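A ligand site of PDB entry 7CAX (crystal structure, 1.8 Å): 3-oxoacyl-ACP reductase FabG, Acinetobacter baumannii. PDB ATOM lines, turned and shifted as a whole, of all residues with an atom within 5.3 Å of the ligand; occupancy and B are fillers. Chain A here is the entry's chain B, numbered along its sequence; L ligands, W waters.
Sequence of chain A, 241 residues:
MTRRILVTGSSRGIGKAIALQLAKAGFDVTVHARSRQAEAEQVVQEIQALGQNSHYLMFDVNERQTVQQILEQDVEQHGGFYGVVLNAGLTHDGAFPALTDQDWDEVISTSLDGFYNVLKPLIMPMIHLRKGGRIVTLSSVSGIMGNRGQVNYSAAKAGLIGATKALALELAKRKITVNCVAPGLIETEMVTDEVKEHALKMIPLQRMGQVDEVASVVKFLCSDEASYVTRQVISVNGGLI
O of Lys 157 lies within hydrogen-bond range of OG of Ser 139. The backbone NH (N) of Phe 59 is in hydrogen-bond range of the backbone carbonyl oxygen (O) of Ala 33, at 3.1 Å. ND2 of Asn 62 is in hydrogen-bond range of OG1 of Thr 110 (3.2 Å). The backbone NH of Leu 138 sits at hydrogen-bond distance from the backbone carbonyl oxygen of Leu 86 (3.0 Å). O of Pro 183 is in hydrogen-bond range of N of Val 141 (3.0 Å). The side-chain amino group of Lys 157 lies within hydrogen-bond range of the backbone carbonyl oxygen of Leu 138 (2.8 Å). A ring nitrogen (ND1) of His 32 sits at hydrogen-bond distance from the backbone NH (N) of Gly 9 (3.0 Å). The backbone NH (N) of Ser 10 lies within hydrogen-bond range of the backbone carbonyl oxygen (O) of His 32.
Water W5 lies within hydrogen-bond range of O15 of the ligand and NE of Arg 34. Water W2 bridges an oxygen (O2) of the ligand (2.6 Å) and the backbone NH of Leu 90 (3.5 Å). Water W3 bridges an oxygen (O9) of the ligand (2.7 Å) and the side-chain hydroxyl (OG1) of Thr 188 (3.0 Å). Water W7 lies within hydrogen-bond range of the backbone carbonyl oxygen (O) of Gly 89 (2.7 Å) and an oxygen (O1) of the ligand (2.8 Å). Water W4 lies within hydrogen-bond range of the side-chain hydroxyl of Ser 140 (2.7 Å), the backbone carbonyl oxygen of Gly 184 (3.3 Å) and the backbone carbonyl oxygen of Pro 183 (3.4 Å).
Residues that only touch the ligand: Ser 10 (3.9 Å), Gly 13 (3.9 Å), His 32 (3.2 Å), Ala 33 (3.5 Å), Phe 59 (3.2 Å), Asn 62 (3.7 Å), Ala 88 (3.3 Å), Thr 110 (3.8 Å), Leu 138 (3.9 Å), Ser 139 (3.2 Å), Ser 140 (3.8 Å), Pro 183 (3.4 Å), Gly 184 (2.9 Å) and Thr 188 (3.7 Å). Of the 35 residues printed, 28 come within 4 Å of the ligand. The nearest printed residue that does not touch the ligand is Leu 185 (4.2 Å).
N of Arg 36 is in hydrogen-bond range of O16 of the ligand, at 2.9 Å. The side-chain carboxylate (OD1) of Asp 60 sits at hydrogen-bond distance from a nitrogen (N3) of the ligand (3.1 Å). O17 of the ligand lies within hydrogen-bond range of OG of Ser 11, 2.5 Å away. The backbone carbonyl oxygen (O) of Asn 87 is in hydrogen-bond range of an oxygen (O12) of the ligand (2.7 Å). An oxygen (O3) of the ligand is in hydrogen-bond range of the backbone NH (N) of Gly 89 (3.5 Å). The backbone NH (N) of Ser 35 is in hydrogen-bond range of an oxygen (O16) of the ligand (2.7 Å). The guanidinium group (NH2) of Arg 12 is in salt-bridge range of an oxygen (O15) of the ligand. OH of Tyr 153 is in hydrogen-bond range of O13 of the ligand (2.4 Å). N of Ile 186 lies within hydrogen-bond range of O14 of the ligand (3.1 Å). O12 of the ligand lies within hydrogen-bond range of NZ of Lys 157 (2.7 Å). An oxygen (O16) of the ligand lies within hydrogen-bond range of the backbone NH of Arg 34. The backbone NH (N) of Ile 14 is in hydrogen-bond range of an oxygen (O8) of the ligand (3.0 Å). The backbone NH (N) of Val 61 is in hydrogen-bond range of a nitrogen (N4) of the ligand, at 2.9 Å. O of Gly 9 sits close to O5 of the ligand, 3.4 Å away.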
ATOM      1  N   GLY A   9      18.815  -3.452   9.054  1.00  0.00           N
ATOM      2  CA  GLY A   9      18.011  -2.568   9.879  1.00  0.00           C
ATOM      3  C   GLY A   9      18.347  -2.642  11.351  1.00  0.00           C
ATOM      4  O   GLY A   9      17.451  -2.693  12.199  1.00  0.00           O
ATOM      5  N   SER A  10      19.646  -2.665  11.672  1.00  0.00           N
ATOM      6  CA  SER A  10      20.078  -2.832  13.048  1.00  0.00           C
ATOM      7  C   SER A  10      20.578  -1.531  13.656  1.00  0.00           C
ATOM      8  O   SER A  10      21.255  -1.561  14.683  1.00  0.00           O
ATOM      9  CB  SER A  10      21.143  -3.931  13.134  1.00  0.00           C
ATOM     10  OG  SER A  10      22.122  -3.825  12.109  1.00  0.00           O
ATOM     11  N   SER A  11      20.267  -0.381  13.037  1.00  0.00           N
ATOM     12  CA  SER A  11      20.616   0.890  13.670  1.00  0.00           C
ATOM     13  C   SER A  11      19.737   1.205  14.868  1.00  0.00           C
ATOM     14  O   SER A  11      20.125   2.022  15.716  1.00  0.00           O
ATOM     15  CB  SER A  11      20.509   2.020  12.642  1.00  0.00           C
ATOM     16  OG  SER A  11      19.183   2.067  12.137  1.00  0.00           O
ATOM     17  N   ARG A  12      18.570   0.573  14.991  1.00  0.00           N
ATOM     18  CA  ARG A  12      17.621   0.955  16.025  1.00  0.00           C
ATOM     19  C   ARG A  12      16.553  -0.112  16.108  1.00  0.00           C
ATOM     20  O   ARG A  12      16.492  -1.011  15.264  1.00  0.00           O
ATOM     21  CB  ARG A  12      16.982   2.324  15.721  1.00  0.00           C
ATOM     22  CG  ARG A  12      16.233   2.364  14.403  1.00  0.00           C
ATOM     23  CD  ARG A  12      16.065   3.810  13.879  1.00  0.00           C
ATOM     24  NE  ARG A  12      15.665   3.848  12.469  1.00  0.00           N
ATOM     25  CZ  ARG A  12      14.410   3.906  12.056  1.00  0.00           C
ATOM     26  NH1 ARG A  12      13.420   3.935  12.947  1.00  0.00           N
ATOM     27  NH2 ARG A  12      14.121   3.931  10.756  1.00  0.00           N
ATOM     28  N   GLY A  13      15.703  -0.001  17.130  1.00  0.00           N
ATOM     29  CA  GLY A  13      14.533  -0.868  17.178  1.00  0.00           C
ATOM     30  C   GLY A  13      14.865  -2.337  17.390  1.00  0.00           C
ATOM     31  O   GLY A  13      15.817  -2.712  18.087  1.00  0.00           O
ATOM     32  N   ILE A  14      14.027  -3.208  16.795  1.00  0.00           N
ATOM     33  CA  ILE A  14      14.220  -4.652  16.979  1.00  0.00           C
ATOM     34  C   ILE A  14      15.575  -5.080  16.422  1.00  0.00           C
ATOM     35  O   ILE A  14      16.287  -5.902  17.033  1.00  0.00           O
ATOM     36  CB  ILE A  14      13.054  -5.424  16.341  1.00  0.00           C
ATOM     37  CG1 ILE A  14      11.757  -5.142  17.112  1.00  0.00           C
ATOM     38  CG2 ILE A  14      13.313  -6.941  16.283  1.00  0.00           C
ATOM     39  CD1 ILE A  14      10.516  -5.712  16.410  1.00  0.00           C
ATOM     40  N   GLY A  15      15.978  -4.531  15.267  1.00  0.00           N
ATOM     41  CA  GLY A  15      17.218  -4.976  14.647  1.00  0.00           C
ATOM     42  C   GLY A  15      18.436  -4.690  15.509  1.00  0.00           C
ATOM     43  O   GLY A  15      19.355  -5.493  15.595  1.00  0.00           O
ATOM     44  N   HIS A  32      23.629  -2.693   9.849  1.00  0.00           N
ATOM     45  CA  HIS A  32      23.215  -2.132   8.572  1.00  0.00           C
ATOM     46  C   HIS A  32      22.104  -1.108   8.801  1.00  0.00           C
ATOM     47  O   HIS A  32      21.276  -1.269   9.701  1.00  0.00           O
ATOM     48  CB  HIS A  32      22.728  -3.213   7.590  1.00  0.00           C
ATOM     49  CG  HIS A  32      21.805  -2.669   6.543  1.00  0.00           C
ATOM     50  ND1 HIS A  32      20.453  -2.537   6.759  1.00  0.00           N
ATOM     51  CD2 HIS A  32      22.054  -2.124   5.332  1.00  0.00           C
ATOM     52  CE1 HIS A  32      19.896  -1.975   5.691  1.00  0.00           C
ATOM     53  NE2 HIS A  32      20.851  -1.703   4.818  1.00  0.00           N
ATOM     54  N   ALA A  33      22.092  -0.072   7.970  1.00  0.00           N
ATOM     55  CA  ALA A  33      21.011   0.907   8.009  1.00  0.00           C
ATOM     56  C   ALA A  33      20.782   1.449   6.600  1.00  0.00           C
ATOM     57  O   ALA A  33      21.646   1.337   5.725  1.00  0.00           O
ATOM     58  CB  ALA A  33      21.323   2.057   8.974  1.00  0.00           C
ATOM     59  N   ARG A  34      19.613   2.051   6.384  1.00  0.00           N
ATOM     60  CA  ARG A  34      19.387   2.703   5.094  1.00  0.00           C
ATOM     61  C   ARG A  34      20.058   4.082   5.056  1.00  0.00           C
ATOM     62  O   ARG A  34      20.753   4.410   4.090  1.00  0.00           O
ATOM     63  CB  ARG A  34      17.895   2.832   4.797  1.00  0.00           C
ATOM     64  CG  ARG A  34      17.626   3.518   3.444  1.00  0.00           C
ATOM     65  CD  ARG A  34      16.151   3.571   3.090  1.00  0.00           C
ATOM     66  NE  ARG A  34      15.437   4.567   3.896  1.00  0.00           N
ATOM     67  CZ  ARG A  34      15.177   5.811   3.491  1.00  0.00           C
ATOM     68  NH1 ARG A  34      15.569   6.220   2.290  1.00  0.00           N
ATOM     69  NH2 ARG A  34      14.532   6.639   4.293  1.00  0.00           N
ATOM     70  N   SER A  35      19.844   4.899   6.079  1.00  0.00           N
ATOM     71  CA  SER A  35      20.420   6.254   6.076  1.00  0.00           C
ATOM     72  C   SER A  35      20.868   6.781   7.437  1.00  0.00           C
ATOM     73  O   SER A  35      21.582   7.784   7.463  1.00  0.00           O
ATOM     74  CB  SER A  35      19.416   7.249   5.486  1.00  0.00           C
ATOM     75  OG  SER A  35      18.246   7.306   6.274  1.00  0.00           O
ATOM     76  N   ARG A  36      20.457   6.182   8.554  1.00  0.00           N
ATOM     77  CA  ARG A  36      20.818   6.721   9.866  1.00  0.00           C
ATOM     78  C   ARG A  36      22.215   6.239  10.253  1.00  0.00           C
ATOM     79  O   ARG A  36      22.419   5.387  11.120  1.00  0.00           O
ATOM     80  CB  ARG A  36      19.762   6.329  10.894  1.00  0.00           C
ATOM     81  CG  ARG A  36      18.427   6.994  10.589  1.00  0.00           C
ATOM     82  CD  ARG A  36      17.654   7.309  11.842  1.00  0.00           C
ATOM     83  NE  ARG A  36      16.224   7.389  11.569  1.00  0.00           N
ATOM     84  CZ  ARG A  36      15.288   7.420  12.509  1.00  0.00           C
ATOM     85  NH1 ARG A  36      15.636   7.383  13.780  1.00  0.00           N
ATOM     86  NH2 ARG A  36      14.006   7.481  12.166  1.00  0.00           N
ATOM     87  N   MET A  58      25.830   0.699   4.730  1.00  0.00           N
ATOM     88  CA  MET A  58      24.677   1.551   4.440  1.00  0.00           C
ATOM     89  C   MET A  58      24.140   1.214   3.055  1.00  0.00           C
ATOM     90  O   MET A  58      24.879   1.287   2.068  1.00  0.00           O
ATOM     91  CB  MET A  58      25.051   3.032   4.508  1.00  0.00           C
ATOM     92  CG  MET A  58      25.758   3.446   5.797  1.00  0.00           C
ATOM     93  SD  MET A  58      24.657   3.397   7.226  1.00  0.00           S
ATOM     94  CE  MET A  58      23.443   4.623   6.762  1.00  0.00           C
ATOM     95  N   PHE A  59      22.872   0.834   2.972  1.00  0.00           N
ATOM     96  CA  PHE A  59      22.246   0.704   1.656  1.00  0.00           C
ATOM     97  C   PHE A  59      20.736   0.563   1.819  1.00  0.00           C
ATOM     98  O   PHE A  59      20.241   0.111   2.846  1.00  0.00           O
ATOM     99  CB  PHE A  59      22.801  -0.480   0.842  1.00  0.00           C
ATOM    100  CG  PHE A  59      22.844  -1.813   1.571  1.00  0.00           C
ATOM    101  CD1 PHE A  59      21.710  -2.601   1.670  1.00  0.00           C
ATOM    102  CD2 PHE A  59      24.052  -2.301   2.071  1.00  0.00           C
ATOM    103  CE1 PHE A  59      21.748  -3.837   2.294  1.00  0.00           C
ATOM    104  CE2 PHE A  59      24.106  -3.555   2.694  1.00  0.00           C
ATOM    105  CZ  PHE A  59      22.953  -4.323   2.818  1.00  0.00           C
ATOM    106  N   ASP A  60      20.033   1.018   0.787  1.00  0.00           N
ATOM    107  CA  ASP A  60      18.626   0.692   0.612  1.00  0.00           C
ATOM    108  C   ASP A  60      18.527  -0.709   0.031  1.00  0.00           C
ATOM    109  O   ASP A  60      19.099  -0.993  -1.023  1.00  0.00           O
ATOM    110  CB  ASP A  60      18.007   1.729  -0.329  1.00  0.00           C
ATOM    111  CG  ASP A  60      16.494   1.655  -0.392  1.00  0.00           C
ATOM    112  OD1 ASP A  60      15.930   0.534  -0.401  1.00  0.00           O
ATOM    113  OD2 ASP A  60      15.872   2.736  -0.462  1.00  0.00           O
ATOM    114  N   VAL A  61      17.791  -1.605   0.703  1.00  0.00           N
ATOM    115  CA  VAL A  61      17.711  -2.987   0.247  1.00  0.00           C
ATOM    116  C   VAL A  61      17.040  -3.111  -1.121  1.00  0.00           C
ATOM    117  O   VAL A  61      17.127  -4.179  -1.753  1.00  0.00           O
ATOM    118  CB  VAL A  61      16.994  -3.896   1.270  1.00  0.00           C
ATOM    119  CG1 VAL A  61      17.746  -3.927   2.592  1.00  0.00           C
ATOM    120  CG2 VAL A  61      15.533  -3.462   1.466  1.00  0.00           C
ATOM    121  N   ASN A  62      16.368  -2.067  -1.586  1.00  0.00           N
ATOM    122  CA  ASN A  62      15.724  -2.098  -2.897  1.00  0.00           C
ATOM    123  C   ASN A  62      16.669  -1.737  -4.040  1.00  0.00           C
ATOM    124  O   ASN A  62      16.276  -1.871  -5.202  1.00  0.00           O
ATOM    125  CB  ASN A  62      14.519  -1.140  -2.931  1.00  0.00           C
ATOM    126  CG  ASN A  62      13.445  -1.541  -1.945  1.00  0.00           C
ATOM    127  OD1 ASN A  62      12.974  -2.672  -1.966  1.00  0.00           O
ATOM    128  ND2 ASN A  62      13.073  -0.615  -1.068  1.00  0.00           N
ATOM    129  N   LEU A  86      17.182 -10.868   8.214  1.00  0.00           N
ATOM    130  CA  LEU A  86      16.505  -9.889   7.378  1.00  0.00           C
ATOM    131  C   LEU A  86      15.455  -9.228   8.251  1.00  0.00           C
ATOM    132  O   LEU A  86      14.310  -9.683   8.352  1.00  0.00           O
ATOM    133  CB  LEU A  86      15.880 -10.563   6.144  1.00  0.00           C
ATOM    134  CG  LEU A  86      16.924 -11.202   5.228  1.00  0.00           C
ATOM    135  CD1 LEU A  86      16.255 -11.922   4.058  1.00  0.00           C
ATOM    136  CD2 LEU A  86      17.862 -10.120   4.709  1.00  0.00           C
ATOM    137  N   ASN A  87      15.876  -8.160   8.932  1.00  0.00           N
ATOM    138  CA  ASN A  87      15.021  -7.476   9.885  1.00  0.00           C
ATOM    139  C   ASN A  87      14.418  -6.195   9.325  1.00  0.00           C
ATOM    140  O   ASN A  87      13.271  -5.889   9.642  1.00  0.00           O
ATOM    141  CB  ASN A  87      15.813  -7.162  11.160  1.00  0.00           C
ATOM    142  CG  ASN A  87      15.140  -6.120  12.034  1.00  0.00           C
ATOM    143  OD1 ASN A  87      14.254  -6.444  12.830  1.00  0.00           O
ATOM    144  ND2 ASN A  87      15.547  -4.862  11.886  1.00  0.00           N
ATOM    145  N   ALA A  88      15.149  -5.441   8.503  1.00  0.00           N
ATOM    146  CA  ALA A  88      14.659  -4.164   8.004  1.00  0.00           C
ATOM    147  C   ALA A  88      13.332  -4.347   7.280  1.00  0.00           C
ATOM    148  O   ALA A  88      13.188  -5.261   6.468  1.00  0.00           O
ATOM    149  CB  ALA A  88      15.680  -3.516   7.043  1.00  0.00           C
ATOM    150  N   GLY A  89      12.360  -3.480   7.594  1.00  0.00           N
ATOM    151  CA  GLY A  89      11.060  -3.560   6.956  1.00  0.00           C
ATOM    152  C   GLY A  89      10.472  -2.170   6.793  1.00  0.00           C
ATOM    153  O   GLY A  89      11.089  -1.162   7.161  1.00  0.00           O
ATOM    154  N   LEU A  90       9.256  -2.118   6.253  1.00  0.00           N
ATOM    155  CA  LEU A  90       8.628  -0.827   6.007  1.00  0.00           C
ATOM    156  C   LEU A  90       7.113  -0.990   5.989  1.00  0.00           C
ATOM    157  O   LEU A  90       6.607  -1.922   5.375  1.00  0.00           O
ATOM    158  CB  LEU A  90       9.127  -0.249   4.671  1.00  0.00           C
ATOM    159  CG  LEU A  90       8.425   1.030   4.210  1.00  0.00           C
ATOM    160  CD1 LEU A  90       8.966   2.217   5.007  1.00  0.00           C
ATOM    161  CD2 LEU A  90       8.566   1.247   2.705  1.00  0.00           C
ATOM    162  N   THR A 110      10.408  -3.688  -0.302  1.00  0.00           N
ATOM    163  CA  THR A 110      11.360  -3.686   0.812  1.00  0.00           C
ATOM    164  C   THR A 110      11.477  -5.087   1.440  1.00  0.00           C
ATOM    165  O   THR A 110      12.575  -5.521   1.793  1.00  0.00           O
ATOM    166  CB  THR A 110      10.966  -2.637   1.853  1.00  0.00           C
ATOM    167  OG1 THR A 110      11.064  -1.331   1.260  1.00  0.00           O
ATOM    168  CG2 THR A 110      11.897  -2.704   3.089  1.00  0.00           C
ATOM    169  N   LEU A 138      12.240 -11.594   9.478  1.00  0.00           N
ATOM    170  CA  LEU A 138      11.282 -11.000  10.414  1.00  0.00           C
ATOM    171  C   LEU A 138       9.975 -10.790   9.657  1.00  0.00           C
ATOM    172  O   LEU A 138       9.908  -9.948   8.763  1.00  0.00           O
ATOM    173  CB  LEU A 138      11.795  -9.674  10.955  1.00  0.00           C
ATOM    174  CG  LEU A 138      12.644  -9.734  12.226  1.00  0.00           C
ATOM    175  CD1 LEU A 138      11.796 -10.093  13.456  1.00  0.00           C
ATOM    176  CD2 LEU A 138      13.807 -10.708  12.074  1.00  0.00           C
ATOM    177  N   SER A 139       8.937 -11.548  10.018  1.00  0.00           N
ATOM    178  CA  SER A 139       7.635 -11.326   9.414  1.00  0.00           C
ATOM    179  C   SER A 139       6.766 -10.546  10.403  1.00  0.00           C
ATOM    180  O   SER A 139       7.250  -9.601  11.037  1.00  0.00           O
ATOM    181  CB  SER A 139       6.959 -12.645   9.038  1.00  0.00           C
ATOM    182  OG  SER A 139       5.736 -12.439   8.342  1.00  0.00           O
ATOM    183  N   SER A 140       5.513 -10.945  10.559  1.00  0.00           N
ATOM    184  CA  SER A 140       4.605 -10.229  11.441  1.00  0.00           C
ATOM    185  C   SER A 140       3.363 -11.081  11.627  1.00  0.00           C
ATOM    186  O   SER A 140       3.024 -11.904  10.769  1.00  0.00           O
ATOM    187  CB  SER A 140       4.200  -8.865  10.849  1.00  0.00           C
ATOM    188  OG  SER A 140       3.066  -8.339  11.528  1.00  0.00           O
ATOM    189  N   VAL A 141       2.660 -10.848  12.735  1.00  0.00           N
ATOM    190  CA  VAL A 141       1.344 -11.465  12.887  1.00  0.00           C
ATOM    191  C   VAL A 141       0.470 -11.136  11.667  1.00  0.00           C
ATOM    192  O   VAL A 141      -0.349 -11.961  11.240  1.00  0.00           O
ATOM    193  CB  VAL A 141       0.696 -11.027  14.219  1.00  0.00           C
ATOM    194  CG1 VAL A 141       0.469  -9.530  14.237  1.00  0.00           C
ATOM    195  CG2 VAL A 141      -0.610 -11.800  14.448  1.00  0.00           C
ATOM    196  N   TYR A 153       1.233  -4.496   3.680  1.00  0.00           N
ATOM    197  CA  TYR A 153       2.172  -5.067   4.645  1.00  0.00           C
ATOM    198  C   TYR A 153       1.900  -6.552   4.909  1.00  0.00           C
ATOM    199  O   TYR A 153       2.837  -7.341   5.079  1.00  0.00           O
ATOM    200  CB  TYR A 153       2.106  -4.267   5.932  1.00  0.00           C
ATOM    201  CG  TYR A 153       3.098  -4.642   6.985  1.00  0.00           C
ATOM    202  CD1 TYR A 153       4.436  -4.299   6.874  1.00  0.00           C
ATOM    203  CD2 TYR A 153       2.675  -5.290   8.142  1.00  0.00           C
ATOM    204  CE1 TYR A 153       5.356  -4.612   7.908  1.00  0.00           C
ATOM    205  CE2 TYR A 153       3.572  -5.601   9.169  1.00  0.00           C
ATOM    206  CZ  TYR A 153       4.890  -5.265   9.039  1.00  0.00           C
ATOM    207  OH  TYR A 153       5.753  -5.589  10.075  1.00  0.00           O
ATOM    208  N   LYS A 157       4.692  -9.347   4.298  1.00  0.00           N
ATOM    209  CA  LYS A 157       5.156 -10.235   5.367  1.00  0.00           C
ATOM    210  C   LYS A 157       4.741 -11.698   5.144  1.00  0.00           C
ATOM    211  O   LYS A 157       5.464 -12.600   5.557  1.00  0.00           O
ATOM    212  CB  LYS A 157       4.647  -9.706   6.709  1.00  0.00           C
ATOM    213  CG  LYS A 157       5.283  -8.339   7.068  1.00  0.00           C
ATOM    214  CD  LYS A 157       6.814  -8.414   6.895  1.00  0.00           C
ATOM    215  CE  LYS A 157       7.540  -7.268   7.558  1.00  0.00           C
ATOM    216  NZ  LYS A 157       9.019  -7.470   7.691  1.00  0.00           N
ATOM    217  N   PRO A 183       6.725 -11.239  14.988  1.00  0.00           N
ATOM    218  CA  PRO A 183       6.326 -10.534  16.200  1.00  0.00           C
ATOM    219  C   PRO A 183       4.881 -10.063  16.118  1.00  0.00           C
ATOM    220  O   PRO A 183       4.335  -9.851  15.033  1.00  0.00           O
ATOM    221  CB  PRO A 183       7.289  -9.335  16.261  1.00  0.00           C
ATOM    222  CG  PRO A 183       8.364  -9.611  15.213  1.00  0.00           C
ATOM    223  CD  PRO A 183       7.732 -10.509  14.196  1.00  0.00           C
ATOM    224  N   GLY A 184       4.274  -9.911  17.291  1.00  0.00           N
ATOM    225  CA  GLY A 184       3.016  -9.204  17.393  1.00  0.00           C
ATOM    226  C   GLY A 184       3.287  -7.724  17.584  1.00  0.00           C
ATOM    227  O   GLY A 184       4.141  -7.153  16.898  1.00  0.00           O
ATOM    228  N   LEU A 185       2.611  -7.089  18.531  1.00  0.00           N
ATOM    229  CA  LEU A 185       2.758  -5.648  18.743  1.00  0.00           C
ATOM    230  C   LEU A 185       3.919  -5.399  19.712  1.00  0.00           C
ATOM    231  O   LEU A 185       3.868  -5.775  20.884  1.00  0.00           O
ATOM    232  CB  LEU A 185       1.454  -5.067  19.276  1.00  0.00           C
ATOM    233  CG  LEU A 185       1.520  -3.564  19.554  1.00  0.00           C
ATOM    234  CD1 LEU A 185       2.019  -2.777  18.328  1.00  0.00           C
ATOM    235  CD2 LEU A 185       0.160  -3.069  20.017  1.00  0.00           C
ATOM    236  N   ILE A 186       4.970  -4.757  19.206  1.00  0.00           N
ATOM    237  CA  ILE A 186       6.202  -4.550  19.940  1.00  0.00           C
ATOM    238  C   ILE A 186       6.354  -3.063  20.226  1.00  0.00           C
ATOM    239  O   ILE A 186       6.106  -2.222  19.346  1.00  0.00           O
ATOM    240  CB  ILE A 186       7.412  -5.088  19.139  1.00  0.00           C
ATOM    241  CG1 ILE A 186       7.176  -6.548  18.740  1.00  0.00           C
ATOM    242  CG2 ILE A 186       8.720  -4.873  19.915  1.00  0.00           C
ATOM    243  CD1 ILE A 186       6.796  -7.468  19.914  1.00  0.00           C
ATOM    244  N   GLU A 187       6.772  -2.727  21.439  1.00  0.00           N
ATOM    245  CA  GLU A 187       7.062  -1.338  21.814  1.00  0.00           C
ATOM    246  C   GLU A 187       8.432  -0.953  21.265  1.00  0.00           C
ATOM    247  O   GLU A 187       9.459  -1.479  21.708  1.00  0.00           O
ATOM    248  CB  GLU A 187       7.024  -1.183  23.333  1.00  0.00           C
ATOM    249  CG  GLU A 187       7.640   0.137  23.818  1.00  0.00           C
ATOM    250  CD  GLU A 187       7.109   0.597  25.175  1.00  0.00           C
ATOM    251  OE1 GLU A 187       6.860  -0.257  26.055  1.00  0.00           O
ATOM    252  OE2 GLU A 187       6.927   1.824  25.360  1.00  0.00           O
ATOM    253  N   THR A 188       8.467  -0.031  20.306  1.00  0.00           N
ATOM    254  CA  THR A 188       9.724   0.493  19.788  1.00  0.00           C
ATOM    255  C   THR A 188       9.916   1.989  20.017  1.00  0.00           C
ATOM    256  O   THR A 188      11.066   2.445  20.094  1.00  0.00           O
ATOM    257  CB  THR A 188       9.871   0.194  18.276  1.00  0.00           C
ATOM    258  OG1 THR A 188       8.701   0.644  17.565  1.00  0.00           O
ATOM    259  CG2 THR A 188      10.116  -1.297  18.020  1.00  0.00           C
HETATM  260  P1  LIG L   1      11.466  -1.100  10.956  1.00  0.00           P
HETATM  261  O1  LIG L   1      10.876   0.272  11.017  1.00  0.00           O
HETATM  262  O2  LIG L   1      10.654  -2.254  10.443  1.00  0.00           O
HETATM  263  O3  LIG L   1      12.851  -1.025  10.035  1.00  0.00           O
HETATM  264  C1  LIG L   1      13.688  -0.091  10.674  1.00  0.00           C
HETATM  265  C2  LIG L   1      15.100  -0.439  10.254  1.00  0.00           C
HETATM  266  O4  LIG L   1      15.047  -0.906   8.913  1.00  0.00           O
HETATM  267  C3  LIG L   1      16.044   0.792  10.367  1.00  0.00           C
HETATM  268  O5  LIG L   1      17.366   0.370  10.719  1.00  0.00           O
HETATM  269  C4  LIG L   1      16.027   1.310   8.918  1.00  0.00           C
HETATM  270  O6  LIG L   1      17.153   1.879   8.527  1.00  0.00           O
HETATM  271  C5  LIG L   1      15.885  -0.044   8.141  1.00  0.00           C
HETATM  272  N1  LIG L   1      15.236   0.138   6.856  1.00  0.00           N
HETATM  273  C6  LIG L   1      13.908   0.553   6.578  1.00  0.00           C
HETATM  274  N2  LIG L   1      13.639   0.585   5.244  1.00  0.00           N
HETATM  275  C7  LIG L   1      14.838   0.185   4.644  1.00  0.00           C
HETATM  276  C8  LIG L   1      15.230   0.010   3.305  1.00  0.00           C
HETATM  277  N3  LIG L   1      14.352   0.256   2.249  1.00  0.00           N
HETATM  278  N4  LIG L   1      16.487  -0.411   2.983  1.00  0.00           N
HETATM  279  C9  LIG L   1      17.332  -0.648   4.050  1.00  0.00           C
HETATM  280  N5  LIG L   1      17.111  -0.534   5.363  1.00  0.00           N
HETATM  281  C10 LIG L   1      15.845  -0.105   5.650  1.00  0.00           C
HETATM  282  O7  LIG L   1      12.074  -1.367  12.520  1.00  0.00           O
HETATM  283  P2  LIG L   1      11.123  -2.162  13.586  1.00  0.00           P
HETATM  284  O8  LIG L   1      12.027  -2.496  14.711  1.00  0.00           O
HETATM  285  O9  LIG L   1       9.768  -1.543  13.849  1.00  0.00           O
HETATM  286  O10 LIG L   1      10.630  -3.725  13.031  1.00  0.00           O
HETATM  287  C11 LIG L   1      11.705  -4.433  12.580  1.00  0.00           C
HETATM  288  C12 LIG L   1      11.166  -5.669  11.861  1.00  0.00           C
HETATM  289  O11 LIG L   1      10.151  -6.329  12.638  1.00  0.00           O
HETATM  290  C13 LIG L   1      10.471  -5.228  10.514  1.00  0.00           C
HETATM  291  O12 LIG L   1      10.634  -6.233   9.538  1.00  0.00           O
HETATM  292  C14 LIG L   1       9.014  -5.089  10.918  1.00  0.00           C
HETATM  293  O13 LIG L   1       8.134  -5.284   9.827  1.00  0.00           O
HETATM  294  C15 LIG L   1       8.916  -6.290  11.906  1.00  0.00           C
HETATM  295  N6  LIG L   1       7.808  -6.101  12.892  1.00  0.00           N
HETATM  296  C16 LIG L   1       7.784  -5.011  13.783  1.00  0.00           C
HETATM  297  C17 LIG L   1       6.776  -4.917  14.703  1.00  0.00           C
HETATM  298  C18 LIG L   1       6.720  -3.791  15.649  1.00  0.00           C
HETATM  299  O14 LIG L   1       5.766  -3.636  16.434  1.00  0.00           O
HETATM  300  N7  LIG L   1       7.759  -2.873  15.662  1.00  0.00           N
HETATM  301  C19 LIG L   1       5.696  -5.919  14.808  1.00  0.00           C
HETATM  302  C20 LIG L   1       5.803  -7.010  13.817  1.00  0.00           C
HETATM  303  C21 LIG L   1       6.805  -7.071  12.934  1.00  0.00           C
HETATM  304  P3  LIG L   1      17.366   3.571   9.084  1.00  0.00           P
HETATM  305  O15 LIG L   1      16.011   4.105   8.751  1.00  0.00           O
HETATM  306  O16 LIG L   1      18.527   4.073   8.237  1.00  0.00           O
HETATM  307  O17 LIG L   1      17.650   3.310  10.549  1.00  0.00           O
HETATM  308  O   HOH W   1       7.412  -1.607  12.020  1.00  0.00           O
HETATM  309  O   HOH W   2       8.189  -2.157   9.562  1.00  0.00           O
HETATM  310  O   HOH W   3       9.644   1.019  14.747  1.00  0.00           O
HETATM  311  O   HOH W   4       2.781  -7.049  13.917  1.00  0.00           O
HETATM  312  O   HOH W   5      14.344   4.053   6.799  1.00  0.00           O
HETATM  313  O   HOH W   6      14.640  -2.717  13.586  1.00  0.00           O
HETATM  314  O   HOH W   7      10.798   1.202   8.420  1.00  0.00           O
